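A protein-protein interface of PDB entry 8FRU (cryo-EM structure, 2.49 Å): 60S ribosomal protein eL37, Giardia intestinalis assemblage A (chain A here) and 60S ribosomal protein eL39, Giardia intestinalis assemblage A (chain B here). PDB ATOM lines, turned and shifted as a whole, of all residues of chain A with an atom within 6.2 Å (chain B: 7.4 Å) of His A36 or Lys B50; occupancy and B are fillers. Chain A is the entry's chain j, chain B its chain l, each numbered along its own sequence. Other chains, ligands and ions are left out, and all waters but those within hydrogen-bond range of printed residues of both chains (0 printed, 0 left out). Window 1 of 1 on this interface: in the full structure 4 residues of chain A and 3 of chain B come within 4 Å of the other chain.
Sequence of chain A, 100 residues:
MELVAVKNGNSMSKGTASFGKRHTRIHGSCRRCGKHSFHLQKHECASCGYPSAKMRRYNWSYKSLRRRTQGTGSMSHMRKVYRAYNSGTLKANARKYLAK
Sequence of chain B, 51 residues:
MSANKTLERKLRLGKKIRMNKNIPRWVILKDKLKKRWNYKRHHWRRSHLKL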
ATOM      1  N   HIS A  27      22.740  -4.404  -6.998  1.00  0.00           N
ATOM      2  CA  HIS A  27      22.265  -4.051  -5.672  1.00  0.00           C
ATOM      3  C   HIS A  27      23.129  -2.939  -5.096  1.00  0.00           C
ATOM      4  O   HIS A  27      24.304  -2.808  -5.437  1.00  0.00           O
ATOM      5  CB  HIS A  27      22.272  -5.275  -4.741  1.00  0.00           C
ATOM      6  CG  HIS A  27      21.256  -6.313  -5.098  1.00  0.00           C
ATOM      7  ND1 HIS A  27      21.522  -7.347  -5.966  1.00  0.00           N
ATOM      8  CD2 HIS A  27      19.969  -6.473  -4.711  1.00  0.00           C
ATOM      9  CE1 HIS A  27      20.446  -8.099  -6.095  1.00  0.00           C
ATOM     10  NE2 HIS A  27      19.492  -7.593  -5.340  1.00  0.00           N
ATOM     11  N   GLY A  28      22.527  -2.128  -4.235  1.00  0.00           N
ATOM     12  CA  GLY A  28      23.226  -1.063  -3.544  1.00  0.00           C
ATOM     13  C   GLY A  28      22.987  -1.116  -2.052  1.00  0.00           C
ATOM     14  O   GLY A  28      22.504  -2.128  -1.546  1.00  0.00           O
ATOM     15  N   SER A  29      23.304  -0.042  -1.337  1.00  0.00           N
ATOM     16  CA  SER A  29      23.149  -0.017   0.112  1.00  0.00           C
ATOM     17  C   SER A  29      21.734   0.383   0.499  1.00  0.00           C
ATOM     18  O   SER A  29      21.201   1.371  -0.005  1.00  0.00           O
ATOM     19  CB  SER A  29      24.147   0.949   0.741  1.00  0.00           C
ATOM     20  OG  SER A  29      25.474   0.586   0.433  1.00  0.00           O
ATOM     21  N   CYS A  30      21.131  -0.387   1.400  1.00  0.00           N
ATOM     22  CA  CYS A  30      19.800  -0.083   1.907  1.00  0.00           C
ATOM     23  C   CYS A  30      19.860   1.048   2.923  1.00  0.00           C
ATOM     24  O   CYS A  30      20.793   1.138   3.719  1.00  0.00           O
ATOM     25  CB  CYS A  30      19.179  -1.327   2.544  1.00  0.00           C
ATOM     26  SG  CYS A  30      17.448  -1.173   3.047  1.00  0.00           S
ATOM     27  N   CYS A  33      18.458  -0.918   6.515  1.00  0.00           N
ATOM     28  CA  CYS A  33      19.353  -1.912   7.087  1.00  0.00           C
ATOM     29  C   CYS A  33      20.799  -1.783   6.626  1.00  0.00           C
ATOM     30  O   CYS A  33      21.681  -2.351   7.270  1.00  0.00           O
ATOM     31  CB  CYS A  33      18.833  -3.330   6.788  1.00  0.00           C
ATOM     32  SG  CYS A  33      19.159  -4.003   5.143  1.00  0.00           S
ATOM     33  N   GLY A  34      21.061  -1.046   5.552  1.00  0.00           N
ATOM     34  CA  GLY A  34      22.417  -0.771   5.093  1.00  0.00           C
ATOM     35  C   GLY A  34      23.230  -1.980   4.690  1.00  0.00           C
ATOM     36  O   GLY A  34      24.425  -2.039   4.990  1.00  0.00           O
ATOM     37  N   LYS A  35      22.625  -2.930   3.974  1.00  0.00           N
ATOM     38  CA  LYS A  35      23.181  -4.274   3.873  1.00  0.00           C
ATOM     39  C   LYS A  35      23.512  -4.711   2.447  1.00  0.00           C
ATOM     40  O   LYS A  35      23.779  -5.893   2.227  1.00  0.00           O
ATOM     41  CB  LYS A  35      22.211  -5.271   4.505  1.00  0.00           C
ATOM     42  CG  LYS A  35      22.830  -6.573   4.912  1.00  0.00           C
ATOM     43  CD  LYS A  35      21.814  -7.488   5.526  1.00  0.00           C
ATOM     44  CE  LYS A  35      22.384  -8.871   5.713  1.00  0.00           C
ATOM     45  NZ  LYS A  35      22.788  -9.481   4.423  1.00  0.00           N
ATOM     46  N   HIS A  36      23.541  -3.803   1.479  1.00  0.00           N
ATOM     47  CA  HIS A  36      23.858  -4.169   0.091  1.00  0.00           C
ATOM     48  C   HIS A  36      22.848  -5.143  -0.509  1.00  0.00           C
ATOM     49  O   HIS A  36      23.215  -6.104  -1.181  1.00  0.00           O
ATOM     50  CB  HIS A  36      25.263  -4.750  -0.040  1.00  0.00           C
ATOM     51  CG  HIS A  36      25.782  -4.725  -1.442  1.00  0.00           C
ATOM     52  ND1 HIS A  36      25.950  -5.870  -2.189  1.00  0.00           N
ATOM     53  CD2 HIS A  36      26.133  -3.697  -2.247  1.00  0.00           C
ATOM     54  CE1 HIS A  36      26.395  -5.551  -3.389  1.00  0.00           C
ATOM     55  NE2 HIS A  36      26.517  -4.238  -3.450  1.00  0.00           N
ATOM     56  N   SER A  37      21.570  -4.886  -0.293  1.00  0.00           N
ATOM     57  CA  SER A  37      20.549  -5.748  -0.864  1.00  0.00           C
ATOM     58  C   SER A  37      19.441  -4.947  -1.527  1.00  0.00           C
ATOM     59  O   SER A  37      18.406  -5.523  -1.863  1.00  0.00           O
ATOM     60  CB  SER A  37      19.957  -6.670   0.200  1.00  0.00           C
ATOM     61  OG  SER A  37      20.955  -7.267   0.996  1.00  0.00           O
ATOM     62  N   PHE A  38      19.625  -3.646  -1.719  1.00  0.00           N
ATOM     63  CA  PHE A  38      18.617  -2.801  -2.343  1.00  0.00           C
ATOM     64  C   PHE A  38      18.729  -2.913  -3.857  1.00  0.00           C
ATOM     65  O   PHE A  38      19.745  -2.531  -4.440  1.00  0.00           O
ATOM     66  CB  PHE A  38      18.780  -1.359  -1.881  1.00  0.00           C
ATOM     67  CG  PHE A  38      17.606  -0.492  -2.198  1.00  0.00           C
ATOM     68  CD1 PHE A  38      16.430  -0.616  -1.489  1.00  0.00           C
ATOM     69  CD2 PHE A  38      17.675   0.443  -3.207  1.00  0.00           C
ATOM     70  CE1 PHE A  38      15.352   0.177  -1.780  1.00  0.00           C
ATOM     71  CE2 PHE A  38      16.599   1.234  -3.500  1.00  0.00           C
ATOM     72  CZ  PHE A  38      15.435   1.102  -2.789  1.00  0.00           C
ATOM     73  N   ARG B   9      27.957   7.468  -1.282  1.00  0.00           N
ATOM     74  CA  ARG B   9      28.952   6.428  -1.497  1.00  0.00           C
ATOM     75  C   ARG B   9      30.333   6.899  -1.077  1.00  0.00           C
ATOM     76  O   ARG B   9      31.104   6.130  -0.496  1.00  0.00           O
ATOM     77  CB  ARG B   9      28.959   5.997  -2.961  1.00  0.00           C
ATOM     78  CG  ARG B   9      27.657   5.400  -3.428  1.00  0.00           C
ATOM     79  CD  ARG B   9      27.876   4.074  -4.123  1.00  0.00           C
ATOM     80  NE  ARG B   9      28.575   4.239  -5.391  1.00  0.00           N
ATOM     81  CZ  ARG B   9      29.419   3.357  -5.906  1.00  0.00           C
ATOM     82  NH1 ARG B   9      29.684   2.214  -5.295  1.00  0.00           N
ATOM     83  NH2 ARG B   9      30.014   3.629  -7.062  1.00  0.00           N
ATOM     84  N   ARG B  12      30.947   6.538   2.748  1.00  0.00           N
ATOM     85  CA  ARG B  12      31.131   5.186   3.255  1.00  0.00           C
ATOM     86  C   ARG B  12      32.494   4.624   2.887  1.00  0.00           C
ATOM     87  O   ARG B  12      33.074   3.866   3.666  1.00  0.00           O
ATOM     88  CB  ARG B  12      30.023   4.275   2.732  1.00  0.00           C
ATOM     89  CG  ARG B  12      28.691   4.472   3.421  1.00  0.00           C
ATOM     90  CD  ARG B  12      28.465   3.426   4.487  1.00  0.00           C
ATOM     91  NE  ARG B  12      27.363   2.536   4.152  1.00  0.00           N
ATOM     92  CZ  ARG B  12      27.230   1.301   4.612  1.00  0.00           C
ATOM     93  NH1 ARG B  12      28.129   0.761   5.413  1.00  0.00           N
ATOM     94  NH2 ARG B  12      26.166   0.591   4.261  1.00  0.00           N
ATOM     95  N   LEU B  13      33.017   4.975   1.714  1.00  0.00           N
ATOM     96  CA  LEU B  13      34.375   4.576   1.369  1.00  0.00           C
ATOM     97  C   LEU B  13      35.404   5.340   2.185  1.00  0.00           C
ATOM     98  O   LEU B  13      36.487   4.819   2.455  1.00  0.00           O
ATOM     99  CB  LEU B  13      34.621   4.776  -0.126  1.00  0.00           C
ATOM    100  CG  LEU B  13      33.851   3.850  -1.071  1.00  0.00           C
ATOM    101  CD1 LEU B  13      33.869   4.384  -2.485  1.00  0.00           C
ATOM    102  CD2 LEU B  13      34.394   2.443  -1.036  1.00  0.00           C
ATOM    103  N   SER B  47      40.411  -7.427  -1.925  1.00  0.00           N
ATOM    104  CA  SER B  47      39.139  -7.275  -1.239  1.00  0.00           C
ATOM    105  C   SER B  47      38.002  -6.973  -2.205  1.00  0.00           C
ATOM    106  O   SER B  47      38.213  -6.600  -3.360  1.00  0.00           O
ATOM    107  CB  SER B  47      39.229  -6.163  -0.193  1.00  0.00           C
ATOM    108  OG  SER B  47      39.043  -4.888  -0.785  1.00  0.00           O
ATOM    109  N   HIS B  48      36.780  -7.154  -1.710  1.00  0.00           N
ATOM    110  CA  HIS B  48      35.568  -6.665  -2.361  1.00  0.00           C
ATOM    111  C   HIS B  48      34.781  -5.918  -1.293  1.00  0.00           C
ATOM    112  O   HIS B  48      34.093  -6.536  -0.482  1.00  0.00           O
ATOM    113  CB  HIS B  48      34.741  -7.795  -2.968  1.00  0.00           C
ATOM    114  CG  HIS B  48      35.557  -8.939  -3.474  1.00  0.00           C
ATOM    115  ND1 HIS B  48      36.271  -8.881  -4.650  1.00  0.00           N
ATOM    116  CD2 HIS B  48      35.770 -10.175  -2.965  1.00  0.00           C
ATOM    117  CE1 HIS B  48      36.895 -10.028  -4.839  1.00  0.00           C
ATOM    118  NE2 HIS B  48      36.606 -10.832  -3.833  1.00  0.00           N
ATOM    119  N   LEU B  49      34.887  -4.591  -1.289  1.00  0.00           N
ATOM    120  CA  LEU B  49      34.219  -3.809  -0.259  1.00  0.00           C
ATOM    121  C   LEU B  49      32.707  -3.801  -0.442  1.00  0.00           C
ATOM    122  O   LEU B  49      31.967  -3.802   0.545  1.00  0.00           O
ATOM    123  CB  LEU B  49      34.771  -2.387  -0.243  1.00  0.00           C
ATOM    124  CG  LEU B  49      36.204  -2.262   0.276  1.00  0.00           C
ATOM    125  CD1 LEU B  49      36.692  -0.827   0.219  1.00  0.00           C
ATOM    126  CD2 LEU B  49      36.315  -2.808   1.682  1.00  0.00           C
ATOM    127  N   LYS B  50      32.230  -3.801  -1.685  1.00  0.00           N
ATOM    128  CA  LYS B  50      30.798  -3.754  -1.975  1.00  0.00           C
ATOM    129  C   LYS B  50      30.150  -2.522  -1.349  1.00  0.00           C
ATOM    130  O   LYS B  50      29.160  -2.611  -0.623  1.00  0.00           O
ATOM    131  CB  LYS B  50      30.100  -5.030  -1.510  1.00  0.00           C
ATOM    132  CG  LYS B  50      30.387  -6.230  -2.376  1.00  0.00           C
ATOM    133  CD  LYS B  50      29.684  -7.458  -1.859  1.00  0.00           C
ATOM    134  CE  LYS B  50      29.964  -8.645  -2.746  1.00  0.00           C
ATOM    135  NZ  LYS B  50      29.183  -9.834  -2.331  1.00  0.00           N
ATOM    136  N   LEU B  51      30.723  -1.360  -1.635  1.00  0.00           N
ATOM    137  CA  LEU B  51      30.207  -0.110  -1.097  1.00  0.00           C
ATOM    138  C   LEU B  51      30.087   0.953  -2.183  1.00  0.00           C
ATOM    139  O   LEU B  51      29.679   2.083  -1.914  1.00  0.00           O
ATOM    140  CB  LEU B  51      31.100   0.395   0.036  1.00  0.00           C
ATOM    141  CG  LEU B  51      30.817  -0.204   1.412  1.00  0.00           C
ATOM    142  CD1 LEU B  51      31.777   0.356   2.441  1.00  0.00           C
ATOM    143  CD2 LEU B  51      29.382   0.054   1.812  1.00  0.00           C
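Among the printed residues, merely in contact across the chains: His A36 with Lys B50 (3.6 Å) and Ser A29 with Arg B12 (3.9 Å).
Of chain B, only Lys B50 (3.6 Å) comes within 4 Å of His A36. Of chain A, only His A36 (3.6 Å) comes within 4 Å of Lys B50. Of the printed residues of chain A, Arg B12 touches Ser A29 (3.9 Å) and Gly A34 (3.2 Å). Of the printed residues of chain B, Gly A34 touches Arg B12. Of the printed residues of chain B, Ser A29 touches Arg B12. The nearest residue of chain A that does not touch Lys B50 is Ser A29 (5.0 Å). The nearest printed residue of chain A that does not touch Arg B12 is Lys A35 (5.0 Å).
The guanidinium group of Arg B12 sits at hydrogen-bond distance from the backbone carbonyl oxygen of Gly A34 (3.2 Å).
The backbone carbonyl oxygen of His A27 is in hydrogen-bond range of a ring nitrogen (NE2) of His A36 (3.3 Å).
Printed residues of chain A that touch a printed residue of chain B: Ser A29, Gly A34 and His A36. Among the printed residues, 3 pairs touch across the chains.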
